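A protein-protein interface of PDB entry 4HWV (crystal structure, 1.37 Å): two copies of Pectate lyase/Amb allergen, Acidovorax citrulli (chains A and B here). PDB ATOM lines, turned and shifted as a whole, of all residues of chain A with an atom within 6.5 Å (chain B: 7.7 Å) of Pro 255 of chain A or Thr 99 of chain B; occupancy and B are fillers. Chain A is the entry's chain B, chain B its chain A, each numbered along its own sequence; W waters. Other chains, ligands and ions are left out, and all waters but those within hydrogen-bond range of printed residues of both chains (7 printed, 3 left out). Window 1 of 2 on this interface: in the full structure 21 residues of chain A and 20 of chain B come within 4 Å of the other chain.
O of His 259 of chain A is in hydrogen-bond range of NH1 of Arg 102 of chain B, 3.2 Å away.
The side-chain hydroxyl (OG1) of Thr 99 of chain B lies close to the backbone NH (N) of Asp 101 of chain B, at 3.4 Å.
N of Arg 102 of chain B is in hydrogen-bond range of OG1 of Thr 99 of chain B.
N of Gln 118 of chain B sits at hydrogen-bond distance from OD1 of Asp 101 of chain B (2.8 Å).
OG of Ser 256 of chain A lies within hydrogen-bond range of N of Trp 258 of chain A (3.1 Å).
O of Trp 258 of chain A sits close to N of Ser 268 of chain A, at 3.5 Å.
Among the printed residues, merely in contact across the chains: His 252 of chain A with Arg 249 of chain B, Ala 253 of chain A with Arg 249 of chain B, Pro 255 of chain A with Thr 99 of chain B, Pro 255 of chain A with Pro 100 of chain B, Ser 256 of chain A with Thr 99 of chain B, Val 257 of chain A with Asp 101 of chain B, His 259 of chain A with Ala 105 of chain B, Ser 268 of chain A with Arg 96 of chain B, Ser 268 of chain A with Thr 99 of chain B and Ser 268 of chain A with Arg 102 of chain B.
Trp 222 of chain A touches none of the printed residues of chain B.
Pro 255 of chain A touches two residues of chain B.
Of the printed residues of chain B, Ser 256 of chain A touches Thr 99 (3.8 Å).
Of the printed residues of chain A, Arg 96 of chain B touches Ser 268.
Of chain A, only Pro 255, Ser 256 and Ser 268 come within 4 Å of Thr 99 of chain B.
Tyr 103 of chain B touches none of the printed residues of chain A.
Of the printed residues of chain A, Ala 105 of chain B touches His 259 (3.4 Å).
The nearest residue of chain B that does not touch Pro 255 of chain A is Tyr 98 of chain B (5.3 Å).
The nearest residue of chain A that does not touch Thr 99 of chain B is Trp 258 of chain A (5.2 Å).
The nearest printed residue of chain A that does not touch Arg 102 of chain B is Trp 258 of chain A (4.8 Å).
Printed residues of chain A that touch a printed residue of chain B: His 252, Ala 253, Pro 255, Ser 256, Val 257, His 259 and Ser 268.
Hydrophobic or aromatic side chains of chain A that line the printed part of chain B: His 252, Ala 253, Pro 255, Val 257 and His 259.
Printed residues of chain B that touch a printed residue of chain A: Arg 96, Thr 99, Pro 100, Asp 101, Arg 102, Ala 105 and Arg 249.
Among the printed residues, 11 pairs touch across the chains.
Among the printed residues, no Asp or Glu carboxylate lies within 4 Å of a Lys or Arg side-chain nitrogen of the other chain.
No position is printed for both chains.
Of the 11 pairs that touch across the chains among the printed residues, none has its exchanged pair printed and touching as well.
Water W5 bridges OD2 of Asp 101 of chain B (2.7 Å) and O of Ser 256 of chain A (2.8 Å).
Water W7 lies within hydrogen-bond range of the side-chain hydroxyl of Thr 99 of chain B (2.7 Å), the backbone carbonyl oxygen of Trp 258 of chain A (2.7 Å) and the backbone carbonyl oxygen of Ser 256 of chain A (2.8 Å).
Water W3 lies within hydrogen-bond range of the backbone carbonyl oxygen of Pro 97 of chain B and the backbone carbonyl oxygen of Ser 268 of chain A.
Water W4 lies within hydrogen-bond range of the backbone carbonyl oxygen (O) of His 252 of chain A (2.8 Å) and the guanidinium group (NH1) of Arg 249 of chain B (3.5 Å).
Water W6 bridges the backbone carbonyl oxygen of Asp 101 of chain B and a ring nitrogen (NE2) of His 259 of chain A.
Water W1 lies within hydrogen-bond range of the guanidinium group of Arg 102 of chain B (2.9 Å), the backbone carbonyl oxygen of His 259 of chain A (3.1 Å) and the backbone NH of Ser 268 of chain A (3.2 Å).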
ATOM      1  N   TRP A 222       1.309 -31.965  29.904  1.00  0.00           N
ATOM      2  CA  TRP A 222       1.585 -31.711  28.485  1.00  0.00           C
ATOM      3  C   TRP A 222       2.842 -30.868  28.364  1.00  0.00           C
ATOM      4  O   TRP A 222       3.015 -29.899  29.096  1.00  0.00           O
ATOM      5  CB  TRP A 222       0.423 -30.950  27.847  1.00  0.00           C
ATOM      6  CG  TRP A 222      -0.798 -31.776  27.649  1.00  0.00           C
ATOM      7  CD1 TRP A 222      -1.882 -31.867  28.490  1.00  0.00           C
ATOM      8  CD2 TRP A 222      -1.076 -32.638  26.534  1.00  0.00           C
ATOM      9  NE1 TRP A 222      -2.823 -32.732  27.955  1.00  0.00           N
ATOM     10  CE2 TRP A 222      -2.348 -33.215  26.758  1.00  0.00           C
ATOM     11  CE3 TRP A 222      -0.382 -32.964  25.357  1.00  0.00           C
ATOM     12  CZ2 TRP A 222      -2.940 -34.099  25.848  1.00  0.00           C
ATOM     13  CZ3 TRP A 222      -0.965 -33.839  24.463  1.00  0.00           C
ATOM     14  CH2 TRP A 222      -2.236 -34.396  24.705  1.00  0.00           C
ATOM     15  N   ASP A 251      -2.670 -19.336  26.880  1.00  0.00           N
ATOM     16  CA  ASP A 251      -2.782 -20.695  27.362  1.00  0.00           C
ATOM     17  C   ASP A 251      -4.169 -21.078  27.841  1.00  0.00           C
ATOM     18  O   ASP A 251      -4.576 -22.218  27.657  1.00  0.00           O
ATOM     19  CB  ASP A 251      -1.801 -20.945  28.506  1.00  0.00           C
ATOM     20  CG  ASP A 251      -0.356 -20.886  28.072  1.00  0.00           C
ATOM     21  OD1 ASP A 251      -0.079 -20.893  26.854  1.00  0.00           O
ATOM     22  OD2 ASP A 251       0.501 -20.871  28.979  1.00  0.00           O
ATOM     23  N   HIS A 252      -4.907 -20.160  28.460  1.00  0.00           N
ATOM     24  CA  HIS A 252      -6.178 -20.598  29.002  1.00  0.00           C
ATOM     25  C   HIS A 252      -7.170 -20.972  27.893  1.00  0.00           C
ATOM     26  O   HIS A 252      -8.176 -21.630  28.169  1.00  0.00           O
ATOM     27  CB  HIS A 252      -6.790 -19.568  29.955  1.00  0.00           C
ATOM     28  CG  HIS A 252      -7.478 -18.435  29.261  1.00  0.00           C
ATOM     29  ND1 HIS A 252      -8.826 -18.453  28.965  1.00  0.00           N
ATOM     30  CD2 HIS A 252      -7.009 -17.247  28.810  1.00  0.00           C
ATOM     31  CE1 HIS A 252      -9.162 -17.316  28.381  1.00  0.00           C
ATOM     32  NE2 HIS A 252      -8.079 -16.560  28.284  1.00  0.00           N
ATOM     33  N   ALA A 253      -6.895 -20.551  26.653  1.00  0.00           N
ATOM     34  CA  ALA A 253      -7.711 -20.928  25.497  1.00  0.00           C
ATOM     35  C   ALA A 253      -7.533 -22.396  25.102  1.00  0.00           C
ATOM     36  O   ALA A 253      -8.266 -22.874  24.243  1.00  0.00           O
ATOM     37  CB  ALA A 253      -7.400 -20.036  24.293  1.00  0.00           C
ATOM     38  N   PHE A 254      -6.579 -23.091  25.715  1.00  0.00           N
ATOM     39  CA  PHE A 254      -6.251 -24.497  25.396  1.00  0.00           C
ATOM     40  C   PHE A 254      -6.264 -25.298  26.697  1.00  0.00           C
ATOM     41  O   PHE A 254      -5.233 -25.697  27.225  1.00  0.00           O
ATOM     42  CB  PHE A 254      -4.927 -24.575  24.641  1.00  0.00           C
ATOM     43  CG  PHE A 254      -4.935 -23.685  23.443  1.00  0.00           C
ATOM     44  CD1 PHE A 254      -5.532 -24.100  22.255  1.00  0.00           C
ATOM     45  CD2 PHE A 254      -4.419 -22.397  23.517  1.00  0.00           C
ATOM     46  CE1 PHE A 254      -5.610 -23.234  21.166  1.00  0.00           C
ATOM     47  CE2 PHE A 254      -4.492 -21.540  22.437  1.00  0.00           C
ATOM     48  CZ  PHE A 254      -5.074 -21.974  21.256  1.00  0.00           C
ATOM     49  N   PRO A 255      -7.479 -25.528  27.224  1.00  0.00           N
ATOM     50  CA  PRO A 255      -7.618 -26.105  28.563  1.00  0.00           C
ATOM     51  C   PRO A 255      -7.354 -27.605  28.560  1.00  0.00           C
ATOM     52  O   PRO A 255      -7.077 -28.209  27.517  1.00  0.00           O
ATOM     53  CB  PRO A 255      -9.079 -25.814  28.909  1.00  0.00           C
ATOM     54  CG  PRO A 255      -9.785 -25.887  27.572  1.00  0.00           C
ATOM     55  CD  PRO A 255      -8.790 -25.264  26.589  1.00  0.00           C
ATOM     56  N   SER A 256      -7.440 -28.225  29.722  1.00  0.00           N
ATOM     57  CA  SER A 256      -7.322 -29.669  29.782  1.00  0.00           C
ATOM     58  C   SER A 256      -8.323 -30.336  28.856  1.00  0.00           C
ATOM     59  O   SER A 256      -9.474 -29.894  28.735  1.00  0.00           O
ATOM     60  CB  SER A 256      -7.587 -30.160  31.206  1.00  0.00           C
ATOM     61  OG  SER A 256      -7.529 -31.574  31.217  1.00  0.00           O
ATOM     62  N   VAL A 257      -7.880 -31.419  28.222  1.00  0.00           N
ATOM     63  CA  VAL A 257      -8.764 -32.252  27.419  1.00  0.00           C
ATOM     64  C   VAL A 257      -9.129 -33.556  28.126  1.00  0.00           C
ATOM     65  O   VAL A 257      -9.755 -34.425  27.530  1.00  0.00           O
ATOM     66  CB  VAL A 257      -8.170 -32.542  26.014  1.00  0.00           C
ATOM     67  CG1 VAL A 257      -8.156 -31.255  25.217  1.00  0.00           C
ATOM     68  CG2 VAL A 257      -6.739 -33.136  26.125  1.00  0.00           C
ATOM     69  N   TRP A 258      -8.715 -33.707  29.385  1.00  0.00           N
ATOM     70  CA  TRP A 258      -9.073 -34.908  30.142  1.00  0.00           C
ATOM     71  C   TRP A 258     -10.288 -34.623  31.017  1.00  0.00           C
ATOM     72  O   TRP A 258     -10.430 -33.522  31.557  1.00  0.00           O
ATOM     73  CB  TRP A 258      -7.940 -35.314  31.071  1.00  0.00           C
ATOM     74  CG  TRP A 258      -6.573 -35.517  30.466  1.00  0.00           C
ATOM     75  CD1 TRP A 258      -5.383 -35.176  31.052  1.00  0.00           C
ATOM     76  CD2 TRP A 258      -6.238 -36.171  29.218  1.00  0.00           C
ATOM     77  NE1 TRP A 258      -4.331 -35.573  30.254  1.00  0.00           N
ATOM     78  CE2 TRP A 258      -4.822 -36.166  29.116  1.00  0.00           C
ATOM     79  CE3 TRP A 258      -6.995 -36.734  28.170  1.00  0.00           C
ATOM     80  CZ2 TRP A 258      -4.142 -36.713  28.013  1.00  0.00           C
ATOM     81  CZ3 TRP A 258      -6.317 -37.275  27.066  1.00  0.00           C
ATOM     82  CH2 TRP A 258      -4.907 -37.263  27.011  1.00  0.00           C
ATOM     83  N   HIS A 259     -11.153 -35.607  31.186  1.00  0.00           N
ATOM     84  CA  HIS A 259     -12.308 -35.405  32.047  1.00  0.00           C
ATOM     85  C   HIS A 259     -12.531 -36.469  33.106  1.00  0.00           C
ATOM     86  O   HIS A 259     -13.533 -36.420  33.804  1.00  0.00           O
ATOM     87  CB  HIS A 259     -13.577 -35.181  31.237  1.00  0.00           C
ATOM     88  CG  HIS A 259     -13.889 -36.282  30.283  1.00  0.00           C
ATOM     89  ND1 HIS A 259     -14.761 -37.304  30.579  1.00  0.00           N
ATOM     90  CD2 HIS A 259     -13.455 -36.510  29.025  1.00  0.00           C
ATOM     91  CE1 HIS A 259     -14.849 -38.117  29.539  1.00  0.00           C
ATOM     92  NE2 HIS A 259     -14.069 -37.652  28.583  1.00  0.00           N
ATOM     93  N   SER A 268      -9.471 -32.623  34.793  1.00  0.00           N
ATOM     94  CA  SER A 268      -9.940 -31.443  34.075  1.00  0.00           C
ATOM     95  C   SER A 268      -9.352 -30.138  34.624  1.00  0.00           C
ATOM     96  O   SER A 268      -9.586 -29.073  34.045  1.00  0.00           O
ATOM     97  CB  SER A 268     -11.469 -31.377  34.044  1.00  0.00           C
ATOM     98  OG  SER A 268     -12.027 -31.000  35.300  1.00  0.00           O
ATOM     99  N   GLY A 269      -8.562 -30.227  35.699  1.00  0.00           N
ATOM    100  CA  GLY A 269      -7.978 -29.036  36.295  1.00  0.00           C
ATOM    101  C   GLY A 269      -6.896 -28.395  35.426  1.00  0.00           C
ATOM    102  O   GLY A 269      -6.333 -29.027  34.521  1.00  0.00           O
ATOM    103  N   PHE A 272      -3.466 -29.586  33.989  1.00  0.00           N
ATOM    104  CA  PHE A 272      -3.494 -30.520  32.866  1.00  0.00           C
ATOM    105  C   PHE A 272      -3.871 -29.830  31.560  1.00  0.00           C
ATOM    106  O   PHE A 272      -4.201 -30.495  30.586  1.00  0.00           O
ATOM    107  CB  PHE A 272      -4.390 -31.708  33.207  1.00  0.00           C
ATOM    108  CG  PHE A 272      -4.039 -32.285  34.542  1.00  0.00           C
ATOM    109  CD1 PHE A 272      -2.816 -32.912  34.711  1.00  0.00           C
ATOM    110  CD2 PHE A 272      -4.873 -32.118  35.646  1.00  0.00           C
ATOM    111  CE1 PHE A 272      -2.429 -33.404  35.943  1.00  0.00           C
ATOM    112  CE2 PHE A 272      -4.495 -32.609  36.873  1.00  0.00           C
ATOM    113  CZ  PHE A 272      -3.265 -33.234  37.034  1.00  0.00           C
ATOM    114  N   LYS A 273      -3.765 -28.503  31.518  1.00  0.00           N
ATOM    115  CA  LYS A 273      -3.995 -27.779  30.272  1.00  0.00           C
ATOM    116  C   LYS A 273      -3.046 -28.270  29.183  1.00  0.00           C
ATOM    117  O   LYS A 273      -1.935 -28.748  29.465  1.00  0.00           O
ATOM    118  CB  LYS A 273      -3.822 -26.269  30.460  1.00  0.00           C
ATOM    119  CG  LYS A 273      -2.387 -25.825  30.794  1.00  0.00           C
ATOM    120  CD  LYS A 273      -2.343 -24.301  30.955  1.00  0.00           C
ATOM    121  CE  LYS A 273      -3.058 -23.838  32.196  1.00  0.00           C
ATOM    122  NZ  LYS A 273      -2.172 -24.070  33.352  1.00  0.00           N
ATOM    123  N   VAL A 274      -3.495 -28.158  27.940  1.00  0.00           N
ATOM    124  CA  VAL A 274      -2.652 -28.545  26.810  1.00  0.00           C
ATOM    125  C   VAL A 274      -1.703 -27.381  26.530  1.00  0.00           C
ATOM    126  O   VAL A 274      -2.039 -26.425  25.825  1.00  0.00           O
ATOM    127  CB  VAL A 274      -3.476 -28.921  25.578  1.00  0.00           C
ATOM    128  CG1 VAL A 274      -2.535 -29.354  24.487  1.00  0.00           C
ATOM    129  CG2 VAL A 274      -4.470 -30.041  25.899  1.00  0.00           C
ATOM    130  N   ASN B  90     -18.105 -19.043  33.571  1.00  0.00           N
ATOM    131  CA  ASN B  90     -17.996 -20.360  32.926  1.00  0.00           C
ATOM    132  C   ASN B  90     -17.465 -21.371  33.934  1.00  0.00           C
ATOM    133  O   ASN B  90     -16.400 -21.973  33.744  1.00  0.00           O
ATOM    134  CB  ASN B  90     -17.123 -20.273  31.668  1.00  0.00           C
ATOM    135  CG  ASN B  90     -17.174 -21.538  30.830  1.00  0.00           C
ATOM    136  OD1 ASN B  90     -18.243 -22.072  30.560  1.00  0.00           O
ATOM    137  ND2 ASN B  90     -16.015 -22.017  30.424  1.00  0.00           N
ATOM    138  N   VAL B  91     -18.221 -21.546  35.020  1.00  0.00           N
ATOM    139  CA  VAL B  91     -17.832 -22.441  36.118  1.00  0.00           C
ATOM    140  C   VAL B  91     -19.035 -23.241  36.600  1.00  0.00           C
ATOM    141  O   VAL B  91     -20.182 -22.810  36.421  1.00  0.00           O
ATOM    142  CB  VAL B  91     -17.207 -21.687  37.303  1.00  0.00           C
ATOM    143  CG1 VAL B  91     -16.026 -20.825  36.831  1.00  0.00           C
ATOM    144  CG2 VAL B  91     -18.248 -20.824  38.024  1.00  0.00           C
ATOM    145  N   ARG B  96     -15.674 -24.726  39.760  1.00  0.00           N
ATOM    146  CA  ARG B  96     -14.619 -25.288  38.920  1.00  0.00           C
ATOM    147  C   ARG B  96     -14.795 -24.810  37.484  1.00  0.00           C
ATOM    148  O   ARG B  96     -15.875 -24.976  36.910  1.00  0.00           O
ATOM    149  CB  ARG B  96     -14.664 -26.813  38.937  1.00  0.00           C
ATOM    150  CG  ARG B  96     -13.589 -27.402  38.026  1.00  0.00           C
ATOM    151  CD  ARG B  96     -13.565 -28.916  38.074  1.00  0.00           C
ATOM    152  NE  ARG B  96     -14.806 -29.499  37.579  1.00  0.00           N
ATOM    153  CZ  ARG B  96     -15.099 -30.794  37.655  1.00  0.00           C
ATOM    154  NH1 ARG B  96     -14.230 -31.631  38.191  1.00  0.00           N
ATOM    155  NH2 ARG B  96     -16.265 -31.245  37.212  1.00  0.00           N
ATOM    156  N   PRO B  97     -13.745 -24.207  36.898  1.00  0.00           N
ATOM    157  CA  PRO B  97     -13.830 -23.782  35.487  1.00  0.00           C
ATOM    158  C   PRO B  97     -14.217 -24.929  34.563  1.00  0.00           C
ATOM    159  O   PRO B  97     -13.646 -26.029  34.606  1.00  0.00           O
ATOM    160  CB  PRO B  97     -12.406 -23.288  35.182  1.00  0.00           C
ATOM    161  CG  PRO B  97     -11.903 -22.829  36.533  1.00  0.00           C
ATOM    162  CD  PRO B  97     -12.448 -23.857  37.512  1.00  0.00           C
ATOM    163  N   TYR B  98     -15.203 -24.668  33.712  1.00  0.00           N
ATOM    164  CA  TYR B  98     -15.596 -25.640  32.698  1.00  0.00           C
ATOM    165  C   TYR B  98     -14.532 -25.769  31.616  1.00  0.00           C
ATOM    166  O   TYR B  98     -13.690 -24.877  31.434  1.00  0.00           O
ATOM    167  CB  TYR B  98     -16.918 -25.220  32.065  1.00  0.00           C
ATOM    168  CG  TYR B  98     -18.104 -25.947  32.638  1.00  0.00           C
ATOM    169  CD1 TYR B  98     -18.401 -27.249  32.230  1.00  0.00           C
ATOM    170  CD2 TYR B  98     -18.935 -25.348  33.576  1.00  0.00           C
ATOM    171  CE1 TYR B  98     -19.494 -27.929  32.733  1.00  0.00           C
ATOM    172  CE2 TYR B  98     -20.041 -26.034  34.096  1.00  0.00           C
ATOM    173  CZ  TYR B  98     -20.310 -27.321  33.667  1.00  0.00           C
ATOM    174  OH  TYR B  98     -21.418 -27.993  34.141  1.00  0.00           O
ATOM    175  N   THR B  99     -14.572 -26.902  30.921  1.00  0.00           N
ATOM    176  CA  THR B  99     -13.807 -27.099  29.702  1.00  0.00           C
ATOM    177  C   THR B  99     -14.772 -27.685  28.692  1.00  0.00           C
ATOM    178  O   THR B  99     -15.828 -28.205  29.074  1.00  0.00           O
ATOM    179  CB  THR B  99     -12.669 -28.126  29.907  1.00  0.00           C
ATOM    180  OG1 THR B  99     -13.262 -29.413  30.120  1.00  0.00           O
ATOM    181  CG2 THR B  99     -11.771 -27.735  31.083  1.00  0.00           C
ATOM    182  N   PRO B 100     -14.433 -27.619  27.398  1.00  0.00           N
ATOM    183  CA  PRO B 100     -15.341 -28.246  26.427  1.00  0.00           C
ATOM    184  C   PRO B 100     -15.502 -29.755  26.685  1.00  0.00           C
ATOM    185  O   PRO B 100     -16.593 -30.311  26.501  1.00  0.00           O
ATOM    186  CB  PRO B 100     -14.636 -27.981  25.097  1.00  0.00           C
ATOM    187  CG  PRO B 100     -13.947 -26.671  25.329  1.00  0.00           C
ATOM    188  CD  PRO B 100     -13.424 -26.771  26.738  1.00  0.00           C
ATOM    189  N   ASP B 101     -14.439 -30.413  27.126  1.00  0.00           N
ATOM    190  CA  ASP B 101     -14.584 -31.830  27.466  1.00  0.00           C
ATOM    191  C   ASP B 101     -15.544 -32.097  28.604  1.00  0.00           C
ATOM    192  O   ASP B 101     -16.240 -33.103  28.599  1.00  0.00           O
ATOM    193  CB  ASP B 101     -13.232 -32.492  27.701  1.00  0.00           C
ATOM    194  CG  ASP B 101     -12.580 -32.865  26.407  1.00  0.00           C
ATOM    195  OD1 ASP B 101     -12.938 -33.940  25.897  1.00  0.00           O
ATOM    196  OD2 ASP B 101     -11.766 -32.072  25.881  1.00  0.00           O
ATOM    197  N   ARG B 102     -15.572 -31.211  29.595  1.00  0.00           N
ATOM    198  CA  ARG B 102     -16.552 -31.324  30.669  1.00  0.00           C
ATOM    199  C   ARG B 102     -17.982 -31.190  30.120  1.00  0.00           C
ATOM    200  O   ARG B 102     -18.880 -31.937  30.497  1.00  0.00           O
ATOM    201  CB  ARG B 102     -16.290 -30.234  31.727  1.00  0.00           C
ATOM    202  CG  ARG B 102     -15.130 -30.525  32.709  1.00  0.00           C
ATOM    203  CD  ARG B 102     -15.705 -30.895  34.091  1.00  0.00           C
ATOM    204  NE  ARG B 102     -16.331 -32.205  33.963  1.00  0.00           N
ATOM    205  CZ  ARG B 102     -15.688 -33.363  34.051  1.00  0.00           C
ATOM    206  NH1 ARG B 102     -14.386 -33.398  34.316  1.00  0.00           N
ATOM    207  NH2 ARG B 102     -16.363 -34.483  33.871  1.00  0.00           N
ATOM    208  N   TYR B 103     -18.191 -30.206  29.246  1.00  0.00           N
ATOM    209  CA  TYR B 103     -19.524 -30.010  28.687  1.00  0.00           C
ATOM    210  C   TYR B 103     -19.977 -31.224  27.880  1.00  0.00           C
ATOM    211  O   TYR B 103     -21.148 -31.611  27.941  1.00  0.00           O
ATOM    212  CB  TYR B 103     -19.590 -28.748  27.828  1.00  0.00           C
ATOM    213  CG  TYR B 103     -19.709 -27.470  28.629  1.00  0.00           C
ATOM    214  CD1 TYR B 103     -20.817 -27.251  29.438  1.00  0.00           C
ATOM    215  CD2 TYR B 103     -18.756 -26.470  28.541  1.00  0.00           C
ATOM    216  CE1 TYR B 103     -20.951 -26.096  30.164  1.00  0.00           C
ATOM    217  CE2 TYR B 103     -18.888 -25.287  29.266  1.00  0.00           C
ATOM    218  CZ  TYR B 103     -19.989 -25.112  30.066  1.00  0.00           C
ATOM    219  OH  TYR B 103     -20.146 -23.951  30.775  1.00  0.00           O
ATOM    220  N   VAL B 104     -19.054 -31.834  27.140  1.00  0.00           N
ATOM    221  CA  VAL B 104     -19.381 -33.048  26.390  1.00  0.00           C
ATOM    222  C   VAL B 104     -19.690 -34.213  27.351  1.00  0.00           C
ATOM    223  O   VAL B 104     -20.712 -34.894  27.209  1.00  0.00           O
ATOM    224  CB  VAL B 104     -18.260 -33.415  25.407  1.00  0.00           C
ATOM    225  CG1 VAL B 104     -18.492 -34.816  24.812  1.00  0.00           C
ATOM    226  CG2 VAL B 104     -18.170 -32.335  24.321  1.00  0.00           C
ATOM    227  N   ALA B 105     -18.820 -34.413  28.340  1.00  0.00           N
ATOM    228  CA  ALA B 105     -18.952 -35.535  29.269  1.00  0.00           C
ATOM    229  C   ALA B 105     -20.176 -35.420  30.165  1.00  0.00           C
ATOM    230  O   ALA B 105     -20.733 -36.431  30.573  1.00  0.00           O
ATOM    231  CB  ALA B 105     -17.690 -35.667  30.128  1.00  0.00           C
ATOM    232  N   GLN B 118     -14.330 -34.081  23.415  1.00  0.00           N
ATOM    233  CA  GLN B 118     -14.545 -32.970  22.514  1.00  0.00           C
ATOM    234  C   GLN B 118     -13.783 -33.194  21.195  1.00  0.00           C
ATOM    235  O   GLN B 118     -14.301 -32.907  20.114  1.00  0.00           O
ATOM    236  CB  GLN B 118     -14.138 -31.659  23.197  1.00  0.00           C
ATOM    237  CG  GLN B 118     -13.864 -30.466  22.270  1.00  0.00           C
ATOM    238  CD  GLN B 118     -15.096 -29.891  21.610  1.00  0.00           C
ATOM    239  OE1 GLN B 118     -16.125 -30.557  21.465  1.00  0.00           O
ATOM    240  NE2 GLN B 118     -14.998 -28.636  21.202  1.00  0.00           N
ATOM    241  N   GLN B 155     -23.791 -25.495  28.310  1.00  0.00           N
ATOM    242  CA  GLN B 155     -23.057 -24.241  28.465  1.00  0.00           C
ATOM    243  C   GLN B 155     -23.997 -23.039  28.570  1.00  0.00           C
ATOM    244  O   GLN B 155     -23.777 -22.159  29.399  1.00  0.00           O
ATOM    245  CB  GLN B 155     -21.999 -24.043  27.349  1.00  0.00           C
ATOM    246  CG  GLN B 155     -21.203 -22.754  27.551  1.00  0.00           C
ATOM    247  CD  GLN B 155     -19.942 -22.674  26.722  1.00  0.00           C
ATOM    248  OE1 GLN B 155     -19.973 -22.934  25.520  1.00  0.00           O
ATOM    249  NE2 GLN B 155     -18.821 -22.352  27.363  1.00  0.00           N
ATOM    250  N   ASP B 208     -18.124 -22.241  23.354  1.00  0.00           N
ATOM    251  CA  ASP B 208     -17.266 -23.369  23.025  1.00  0.00           C
ATOM    252  C   ASP B 208     -17.840 -24.311  21.985  1.00  0.00           C
ATOM    253  O   ASP B 208     -17.139 -25.222  21.555  1.00  0.00           O
ATOM    254  CB  ASP B 208     -16.935 -24.141  24.291  1.00  0.00           C
ATOM    255  CG  ASP B 208     -15.843 -23.470  25.069  1.00  0.00           C
ATOM    256  OD1 ASP B 208     -14.696 -23.426  24.565  1.00  0.00           O
ATOM    257  OD2 ASP B 208     -16.119 -22.980  26.166  1.00  0.00           O
ATOM    258  N   PHE B 209     -19.093 -24.072  21.584  1.00  0.00           N
ATOM    259  CA  PHE B 209     -19.793 -24.971  20.659  1.00  0.00           C
ATOM    260  C   PHE B 209     -20.494 -24.196  19.546  1.00  0.00           C
ATOM    261  O   PHE B 209     -21.708 -24.313  19.365  1.00  0.00           O
ATOM    262  CB  PHE B 209     -20.749 -25.874  21.448  1.00  0.00           C
ATOM    263  CG  PHE B 209     -20.017 -26.741  22.431  1.00  0.00           C
ATOM    264  CD1 PHE B 209     -19.340 -27.877  21.983  1.00  0.00           C
ATOM    265  CD2 PHE B 209     -19.938 -26.392  23.776  1.00  0.00           C
ATOM    266  CE1 PHE B 209     -18.597 -28.643  22.858  1.00  0.00           C
ATOM    267  CE2 PHE B 209     -19.191 -27.166  24.656  1.00  0.00           C
ATOM    268  CZ  PHE B 209     -18.518 -28.293  24.192  1.00  0.00           C
ATOM    269  N   ARG B 249      -9.053 -13.605  24.017  1.00  0.00           N
ATOM    270  CA  ARG B 249      -9.333 -14.560  22.952  1.00  0.00           C
ATOM    271  C   ARG B 249      -9.939 -13.827  21.766  1.00  0.00           C
ATOM    272  O   ARG B 249     -11.157 -13.866  21.528  1.00  0.00           O
ATOM    273  CB  ARG B 249     -10.245 -15.688  23.436  1.00  0.00           C
ATOM    274  CG  ARG B 249      -9.493 -16.701  24.300  1.00  0.00           C
ATOM    275  CD  ARG B 249     -10.331 -17.938  24.645  1.00  0.00           C
ATOM    276  NE  ARG B 249     -11.414 -17.579  25.549  1.00  0.00           N
ATOM    277  CZ  ARG B 249     -12.199 -18.468  26.152  1.00  0.00           C
ATOM    278  NH1 ARG B 249     -12.059 -19.780  25.922  1.00  0.00           N
ATOM    279  NH2 ARG B 249     -13.105 -18.035  27.013  1.00  0.00           N
HETATM  280  O   HOH W   1     -12.003 -34.411  35.596  1.00  0.00           O
HETATM  281  O   HOH W   2     -10.715 -21.533  23.799  1.00  0.00           O
HETATM  282  O   HOH W   3     -11.073 -26.890  35.123  1.00  0.00           O
HETATM  283  O   HOH W   4     -10.766 -22.480  27.643  1.00  0.00           O
HETATM  284  O   HOH W   5     -11.398 -29.553  26.710  1.00  0.00           O
HETATM  285  O   HOH W   6     -15.546 -35.261  26.963  1.00  0.00           O
HETATM  286  O   HOH W   7     -11.248 -31.161  30.475  1.00  0.00           O
